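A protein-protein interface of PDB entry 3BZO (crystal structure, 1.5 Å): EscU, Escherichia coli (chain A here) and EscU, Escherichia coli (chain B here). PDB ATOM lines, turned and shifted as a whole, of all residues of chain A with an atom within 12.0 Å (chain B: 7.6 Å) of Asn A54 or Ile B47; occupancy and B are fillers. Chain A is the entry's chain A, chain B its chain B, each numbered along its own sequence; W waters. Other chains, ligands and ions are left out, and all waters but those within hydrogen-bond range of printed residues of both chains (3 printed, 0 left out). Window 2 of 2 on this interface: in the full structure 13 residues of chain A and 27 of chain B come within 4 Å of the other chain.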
ATOM      1  N   VAL A  50      -2.023 -37.359 -32.761  1.00  0.00           N
ATOM      2  CA  VAL A  50      -0.744 -36.723 -32.506  1.00  0.00           C
ATOM      3  C   VAL A  50      -0.858 -35.826 -31.289  1.00  0.00           C
ATOM      4  O   VAL A  50      -1.924 -35.283 -31.038  1.00  0.00           O
ATOM      5  CB  VAL A  50      -0.298 -35.909 -33.733  1.00  0.00           C
ATOM      6  CG1 VAL A  50      -1.317 -34.790 -34.034  1.00  0.00           C
ATOM      7  CG2 VAL A  50       1.119 -35.370 -33.549  1.00  0.00           C
ATOM      8  N   ILE A  51       0.240 -35.712 -30.533  1.00  0.00           N
ATOM      9  CA  ILE A  51       0.324 -34.823 -29.385  1.00  0.00           C
ATOM     10  C   ILE A  51       1.273 -33.699 -29.752  1.00  0.00           C
ATOM     11  O   ILE A  51       2.358 -33.966 -30.261  1.00  0.00           O
ATOM     12  CB  ILE A  51       0.953 -35.514 -28.158  1.00  0.00           C
ATOM     13  CG1 ILE A  51       0.250 -36.823 -27.826  1.00  0.00           C
ATOM     14  CG2 ILE A  51       1.007 -34.565 -26.951  1.00  0.00           C
ATOM     15  CD1 ILE A  51      -1.183 -36.698 -27.736  1.00  0.00           C
ATOM     16  N   VAL A  52       0.869 -32.463 -29.512  1.00  0.00           N
ATOM     17  CA  VAL A  52       1.767 -31.310 -29.647  1.00  0.00           C
ATOM     18  C   VAL A  52       2.103 -30.823 -28.252  1.00  0.00           C
ATOM     19  O   VAL A  52       1.213 -30.623 -27.431  1.00  0.00           O
ATOM     20  CB  VAL A  52       1.129 -30.157 -30.440  1.00  0.00           C
ATOM     21  CG1 VAL A  52       2.197 -29.134 -30.834  1.00  0.00           C
ATOM     22  CG2 VAL A  52       0.472 -30.680 -31.669  1.00  0.00           C
ATOM     23  N   LYS A  53       3.393 -30.599 -28.010  1.00  0.00           N
ATOM     24  CA  LYS A  53       3.854 -30.152 -26.712  1.00  0.00           C
ATOM     25  C   LYS A  53       4.776 -28.959 -26.874  1.00  0.00           C
ATOM     26  O   LYS A  53       5.288 -28.704 -27.969  1.00  0.00           O
ATOM     27  CB  LYS A  53       4.574 -31.270 -25.951  1.00  0.00           C
ATOM     28  CG  LYS A  53       5.913 -31.715 -26.549  1.00  0.00           C
ATOM     29  CD  LYS A  53       6.588 -32.829 -25.713  1.00  0.00           C
ATOM     30  CE  LYS A  53       7.196 -32.283 -24.417  1.00  0.00           C
ATOM     31  NZ  LYS A  53       8.364 -31.368 -24.671  1.00  0.00           N
ATOM     32  N   ASN A  54       4.943 -28.215 -25.787  1.00  0.00           N
ATOM     33  CA  ASN A  54       5.947 -27.170 -25.724  1.00  0.00           C
ATOM     34  C   ASN A  54       7.200 -27.735 -25.079  1.00  0.00           C
ATOM     35  O   ASN A  54       7.363 -28.951 -25.033  1.00  0.00           O
ATOM     36  CB  ASN A  54       5.433 -25.945 -24.964  1.00  0.00           C
ATOM     37  CG  ASN A  54       5.260 -26.197 -23.488  1.00  0.00           C
ATOM     38  OD1 ASN A  54       5.203 -27.349 -23.042  1.00  0.00           O
ATOM     39  ND2 ASN A  54       5.116 -25.124 -22.721  1.00  0.00           N
ATOM     40  OXT ASN A  54       8.056 -27.016 -24.566  1.00  0.00           O
ATOM     41  N   THR B   2       6.080 -23.693 -17.724  1.00  0.00           N
ATOM     42  CA  THR B   2       4.759 -24.382 -17.703  1.00  0.00           C
ATOM     43  C   THR B   2       4.632 -25.350 -18.868  1.00  0.00           C
ATOM     44  O   THR B   2       4.531 -24.942 -20.015  1.00  0.00           O
ATOM     45  CB  THR B   2       3.581 -23.396 -17.790  1.00  0.00           C
ATOM     46  OG1 THR B   2       3.634 -22.473 -16.699  1.00  0.00           O
ATOM     47  CG2 THR B   2       2.255 -24.151 -17.755  1.00  0.00           C
ATOM     48  N   HIS B   3       4.575 -26.633 -18.562  1.00  0.00           N
ATOM     49  CA  HIS B   3       4.475 -27.664 -19.580  1.00  0.00           C
ATOM     50  C   HIS B   3       3.049 -27.732 -20.106  1.00  0.00           C
ATOM     51  O   HIS B   3       2.101 -27.650 -19.333  1.00  0.00           O
ATOM     52  CB  HIS B   3       4.853 -29.018 -18.986  1.00  0.00           C
ATOM     53  CG  HIS B   3       6.312 -29.164 -18.667  1.00  0.00           C
ATOM     54  ND1 HIS B   3       6.991 -28.311 -17.821  1.00  0.00           N
ATOM     55  CD2 HIS B   3       7.218 -30.082 -19.081  1.00  0.00           C
ATOM     56  CE1 HIS B   3       8.250 -28.707 -17.719  1.00  0.00           C
ATOM     57  NE2 HIS B   3       8.411 -29.779 -18.475  1.00  0.00           N
ATOM     58  N   ILE B   4       2.921 -27.919 -21.421  1.00  0.00           N
ATOM     59  CA  ILE B   4       1.602 -28.086 -22.012  1.00  0.00           C
ATOM     60  C   ILE B   4       1.632 -29.199 -23.042  1.00  0.00           C
ATOM     61  O   ILE B   4       2.647 -29.489 -23.667  1.00  0.00           O
ATOM     62  CB  ILE B   4       1.028 -26.793 -22.614  1.00  0.00           C
ATOM     63  CG1 ILE B   4       2.029 -26.151 -23.566  1.00  0.00           C
ATOM     64  CG2 ILE B   4       0.637 -25.813 -21.508  1.00  0.00           C
ATOM     65  CD1 ILE B   4       1.492 -24.916 -24.273  1.00  0.00           C
ATOM     66  N   ALA B   5       0.497 -29.890 -23.135  1.00  0.00           N
ATOM     67  CA  ALA B   5       0.312 -30.952 -24.115  1.00  0.00           C
ATOM     68  C   ALA B   5      -1.105 -30.877 -24.653  1.00  0.00           C
ATOM     69  O   ALA B   5      -2.066 -30.693 -23.890  1.00  0.00           O
ATOM     70  CB  ALA B   5       0.575 -32.345 -23.504  1.00  0.00           C
ATOM     71  N   ILE B   6      -1.208 -31.005 -25.970  1.00  0.00           N
ATOM     72  CA  ILE B   6      -2.452 -30.931 -26.713  1.00  0.00           C
ATOM     73  C   ILE B   6      -2.587 -32.202 -27.511  1.00  0.00           C
ATOM     74  O   ILE B   6      -1.718 -32.535 -28.322  1.00  0.00           O
ATOM     75  CB  ILE B   6      -2.422 -29.782 -27.741  1.00  0.00           C
ATOM     76  CG1 ILE B   6      -1.988 -28.459 -27.095  1.00  0.00           C
ATOM     77  CG2 ILE B   6      -3.780 -29.644 -28.425  1.00  0.00           C
ATOM     78  CD1 ILE B   6      -2.936 -27.939 -26.135  1.00  0.00           C
ATOM     79  N   GLY B  24      -3.524 -30.690 -21.379  1.00  0.00           N
ATOM     80  CA  GLY B  24      -2.993 -30.678 -20.038  1.00  0.00           C
ATOM     81  C   GLY B  24      -1.926 -29.631 -19.870  1.00  0.00           C
ATOM     82  O   GLY B  24      -1.242 -29.281 -20.822  1.00  0.00           O
ATOM     83  N   ASP B  26       1.203 -28.621 -16.794  1.00  0.00           N
ATOM     84  CA  ASP B  26       1.893 -29.059 -15.590  1.00  0.00           C
ATOM     85  C   ASP B  26       1.825 -30.585 -15.438  1.00  0.00           C
ATOM     86  O   ASP B  26       2.156 -31.298 -16.370  1.00  0.00           O
ATOM     87  CB  ASP B  26       1.324 -28.328 -14.373  1.00  0.00           C
ATOM     88  CG  ASP B  26       1.487 -26.812 -14.467  1.00  0.00           C
ATOM     89  OD1 ASP B  26       2.566 -26.352 -14.907  1.00  0.00           O
ATOM     90  OD2 ASP B  26       0.552 -26.074 -14.076  1.00  0.00           O
ATOM     91  N   ALA B  29       0.069 -32.467 -18.194  1.00  0.00           N
ATOM     92  CA  ALA B  29       0.832 -32.535 -19.430  1.00  0.00           C
ATOM     93  C   ALA B  29       1.859 -33.675 -19.361  1.00  0.00           C
ATOM     94  O   ALA B  29       2.040 -34.411 -20.332  1.00  0.00           O
ATOM     95  CB  ALA B  29       1.514 -31.195 -19.737  1.00  0.00           C
ATOM     96  N   ILE B  33       2.022 -37.100 -21.848  1.00  0.00           N
ATOM     97  CA  ILE B  33       3.200 -37.497 -22.598  1.00  0.00           C
ATOM     98  C   ILE B  33       3.604 -38.931 -22.251  1.00  0.00           C
ATOM     99  O   ILE B  33       3.987 -39.692 -23.134  1.00  0.00           O
ATOM    100  CB  ILE B  33       4.351 -36.486 -22.392  1.00  0.00           C
ATOM    101  CG1 ILE B  33       3.988 -35.168 -23.096  1.00  0.00           C
ATOM    102  CG2 ILE B  33       5.663 -37.050 -22.905  1.00  0.00           C
ATOM    103  CD1 ILE B  33       4.648 -33.929 -22.505  1.00  0.00           C
ATOM    104  N   VAL B  43       4.612 -37.677 -30.663  1.00  0.00           N
ATOM    105  CA  VAL B  43       4.662 -36.437 -29.891  1.00  0.00           C
ATOM    106  C   VAL B  43       5.607 -35.488 -30.607  1.00  0.00           C
ATOM    107  O   VAL B  43       6.765 -35.824 -30.827  1.00  0.00           O
ATOM    108  CB  VAL B  43       5.161 -36.647 -28.446  1.00  0.00           C
ATOM    109  CG1 VAL B  43       5.351 -35.301 -27.735  1.00  0.00           C
ATOM    110  CG2 VAL B  43       4.208 -37.546 -27.649  1.00  0.00           C
ATOM    111  N   ILE B  44       5.104 -34.311 -30.957  1.00  0.00           N
ATOM    112  CA  ILE B  44       5.866 -33.300 -31.668  1.00  0.00           C
ATOM    113  C   ILE B  44       6.012 -32.075 -30.788  1.00  0.00           C
ATOM    114  O   ILE B  44       5.027 -31.545 -30.274  1.00  0.00           O
ATOM    115  CB  ILE B  44       5.163 -32.892 -32.976  1.00  0.00           C
ATOM    116  CG1 ILE B  44       4.989 -34.120 -33.872  1.00  0.00           C
ATOM    117  CG2 ILE B  44       5.940 -31.804 -33.676  1.00  0.00           C
ATOM    118  CD1 ILE B  44       4.320 -33.843 -35.193  1.00  0.00           C
ATOM    119  N   GLU B  45       7.249 -31.603 -30.628  1.00  0.00           N
ATOM    120  CA  GLU B  45       7.487 -30.362 -29.899  1.00  0.00           C
ATOM    121  C   GLU B  45       7.461 -29.171 -30.852  1.00  0.00           C
ATOM    122  O   GLU B  45       8.237 -29.096 -31.805  1.00  0.00           O
ATOM    123  CB  GLU B  45       8.833 -30.392 -29.172  1.00  0.00           C
ATOM    124  CG  GLU B  45       9.113 -29.120 -28.403  1.00  0.00           C
ATOM    125  CD  GLU B  45      10.385 -29.194 -27.590  1.00  0.00           C
ATOM    126  OE1 GLU B  45      10.558 -30.187 -26.853  1.00  0.00           O
ATOM    127  OE2 GLU B  45      11.192 -28.252 -27.687  1.00  0.00           O
ATOM    128  N   ASP B  46       6.552 -28.247 -30.588  1.00  0.00           N
ATOM    129  CA  ASP B  46       6.403 -27.044 -31.389  1.00  0.00           C
ATOM    130  C   ASP B  46       5.817 -26.026 -30.437  1.00  0.00           C
ATOM    131  O   ASP B  46       4.610 -26.013 -30.174  1.00  0.00           O
ATOM    132  CB  ASP B  46       5.496 -27.296 -32.594  1.00  0.00           C
ATOM    133  CG  ASP B  46       5.412 -26.096 -33.533  1.00  0.00           C
ATOM    134  OD1 ASP B  46       5.425 -24.939 -33.072  1.00  0.00           O
ATOM    135  OD2 ASP B  46       5.297 -26.318 -34.760  1.00  0.00           O
ATOM    136  N   ILE B  47       6.695 -25.203 -29.871  1.00  0.00           N
ATOM    137  CA  ILE B  47       6.304 -24.389 -28.738  1.00  0.00           C
ATOM    138  C   ILE B  47       5.291 -23.306 -29.142  1.00  0.00           C
ATOM    139  O   ILE B  47       4.252 -23.171 -28.496  1.00  0.00           O
ATOM    140  CB  ILE B  47       7.569 -23.818 -28.035  1.00  0.00           C
ATOM    141  CG1 ILE B  47       8.367 -24.967 -27.401  1.00  0.00           C
ATOM    142  CG2 ILE B  47       7.176 -22.798 -26.995  1.00  0.00           C
ATOM    143  CD1 ILE B  47       9.831 -24.634 -27.103  1.00  0.00           C
ATOM    144  N   PRO B  48       5.567 -22.540 -30.214  1.00  0.00           N
ATOM    145  CA  PRO B  48       4.530 -21.574 -30.608  1.00  0.00           C
ATOM    146  C   PRO B  48       3.152 -22.184 -30.944  1.00  0.00           C
ATOM    147  O   PRO B  48       2.110 -21.638 -30.552  1.00  0.00           O
ATOM    148  CB  PRO B  48       5.143 -20.868 -31.820  1.00  0.00           C
ATOM    149  CG  PRO B  48       6.616 -21.054 -31.653  1.00  0.00           C
ATOM    150  CD  PRO B  48       6.755 -22.442 -31.077  1.00  0.00           C
ATOM    151  N   LEU B  49       3.136 -23.321 -31.638  1.00  0.00           N
ATOM    152  CA  LEU B  49       1.880 -23.982 -31.957  1.00  0.00           C
ATOM    153  C   LEU B  49       1.204 -24.521 -30.693  1.00  0.00           C
ATOM    154  O   LEU B  49      -0.004 -24.363 -30.512  1.00  0.00           O
ATOM    155  CB  LEU B  49       2.098 -25.103 -32.977  1.00  0.00           C
ATOM    156  CG  LEU B  49       0.830 -25.818 -33.441  1.00  0.00           C
ATOM    157  CD1 LEU B  49      -0.205 -24.863 -34.064  1.00  0.00           C
ATOM    158  CD2 LEU B  49       1.232 -26.922 -34.400  1.00  0.00           C
ATOM    159  N   ALA B  50       1.969 -25.164 -29.829  1.00  0.00           N
ATOM    160  CA  ALA B  50       1.372 -25.705 -28.600  1.00  0.00           C
ATOM    161  C   ALA B  50       0.746 -24.600 -27.750  1.00  0.00           C
ATOM    162  O   ALA B  50      -0.376 -24.746 -27.277  1.00  0.00           O
ATOM    163  CB  ALA B  50       2.399 -26.461 -27.804  1.00  0.00           C
ATOM    164  N   ARG B  51       1.459 -23.494 -27.557  1.00  0.00           N
ATOM    165  CA  ARG B  51       0.905 -22.403 -26.761  1.00  0.00           C
ATOM    166  C   ARG B  51      -0.371 -21.841 -27.382  1.00  0.00           C
ATOM    167  O   ARG B  51      -1.348 -21.534 -26.691  1.00  0.00           O
ATOM    168  CB  ARG B  51       1.940 -21.289 -26.609  1.00  0.00           C
ATOM    169  CG  ARG B  51       3.054 -21.613 -25.631  1.00  0.00           C
ATOM    170  CD  ARG B  51       3.686 -20.347 -25.067  1.00  0.00           C
ATOM    171  NE  ARG B  51       4.408 -19.589 -26.086  1.00  0.00           N
ATOM    172  CZ  ARG B  51       5.735 -19.481 -26.160  1.00  0.00           C
ATOM    173  NH1 ARG B  51       6.510 -20.084 -25.276  1.00  0.00           N
ATOM    174  NH2 ARG B  51       6.284 -18.762 -27.132  1.00  0.00           N
ATOM    175  N   SER B  52      -0.364 -21.690 -28.692  1.00  0.00           N
ATOM    176  CA  SER B  52      -1.503 -21.107 -29.385  1.00  0.00           C
ATOM    177  C   SER B  52      -2.709 -22.046 -29.356  1.00  0.00           C
ATOM    178  O   SER B  52      -3.842 -21.606 -29.115  1.00  0.00           O
ATOM    179  CB  SER B  52      -1.114 -20.770 -30.827  1.00  0.00           C
ATOM    180  OG  SER B  52      -2.158 -20.082 -31.484  1.00  0.00           O
ATOM    181  N   LEU B  53      -2.493 -23.327 -29.639  1.00  0.00           N
ATOM    182  CA  LEU B  53      -3.581 -24.300 -29.507  1.00  0.00           C
ATOM    183  C   LEU B  53      -4.144 -24.315 -28.099  1.00  0.00           C
ATOM    184  O   LEU B  53      -5.350 -24.353 -27.921  1.00  0.00           O
ATOM    185  CB  LEU B  53      -3.117 -25.711 -29.882  1.00  0.00           C
ATOM    186  CG  LEU B  53      -2.987 -25.993 -31.374  1.00  0.00           C
ATOM    187  CD1 LEU B  53      -2.174 -27.268 -31.581  1.00  0.00           C
ATOM    188  CD2 LEU B  53      -4.353 -26.121 -32.045  1.00  0.00           C
HETATM  189  O   HOH W   1      10.741 -27.730 -24.748  1.00  0.00           O
HETATM  190  O   HOH W   2       5.276 -30.249 -22.474  1.00  0.00           O
HETATM  191  O   HOH W   3       6.131 -22.309 -23.428  1.00  0.00           O
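O of His B3 sits at hydrogen-bond distance from N of Asp B26 (2.9 Å).
O of Ala B5 lies within hydrogen-bond range of N of Gly B24 (2.9 Å).
The side-chain carboxylate (OD1) of Asp B46 sits at hydrogen-bond distance from the backbone NH (N) of Leu B49, 3.1 Å away.
O of Ile A51 sits at hydrogen-bond distance from N of Ile B44, at 2.9 Å.
The backbone NH of Val A52 sits at hydrogen-bond distance from the backbone carbonyl oxygen of Ile B6 (2.8 Å).
The backbone NH (N) of Lys A53 lies within hydrogen-bond range of the backbone carbonyl oxygen (O) of Ile B44.
The side-chain amino group (NZ) of Lys A53 is in salt-bridge range of the side-chain carboxylate (OE1) of Glu B45.
The backbone NH of Asp B46 is in hydrogen-bond range of the backbone carbonyl oxygen of Lys A53 (2.9 Å).
O of Thr B2 sits at hydrogen-bond distance from ND2 of Asn A54.
OD1 of Asn A54 is in hydrogen-bond range of N of Ile B4 (2.9 Å).
Printed residues of chain B within 4 Å of Asn A54: Thr B2, His B3, Ile B4, Glu B45, Ile B47 and Ala B50.
Ile B47 touches one residue of chain A.
Pro B48 touches none of the printed residues of chain A.
Of the printed residues of chain A, Glu B45 touches Lys A53 (3.3 Å) and Asn A54 (3.8 Å).
Of the printed residues of chain A, Val B43 touches Ile A51 (3.4 Å) and Lys A53 (3.4 Å).
Printed residues of chain A within 4 Å of Ile B44: Val A50 (3.9 Å), Ile A51 (2.9 Å), Val A52 (3.3 Å) and Lys A53 (2.9 Å).
The nearest printed residue of chain A that does not touch Ile B6 is Lys A53 (5.0 Å).
Val A50 touches Ile B6.
Ile B44 touches Val A50.
CA of Val B43 touches O of Ile A51, at 3.4 Å.
Ala B5 touches Val A52.
CA of Val A52 touches O of Ile B44, 3.3 Å away.
CA of Lys A53 touches O of Ile B4, 3.3 Å away.
Lys A53 touches Ile B33.
CD of Lys A53 touches CG1 of Val B43, 3.4 Å away.
CA of His B3 touches OD1 of Asn A54, at 3.6 Å.
N of Asn A54 touches CB of Ala B50 (3.7 Å).
Of the 5 printed residues of chain A, 5 touch a printed residue of chain B.
Of the 20 printed residues of chain B, 12 touch a printed residue of chain A.
Water W1 lies within hydrogen-bond range of the chain-end carboxylate (OXT) of Asn A54 (2.8 Å) and the side-chain carboxylate (OE2) of Glu B45 (3.0 Å).
Water W3 bridges the guanidinium group of Arg B51 (2.9 Å) and the side-chain amide nitrogen of Asn A54 (3.1 Å).
Water W2 lies within hydrogen-bond range of OD1 of Asn A54 (3.0 Å) and O of Ile B4 (3.0 Å).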
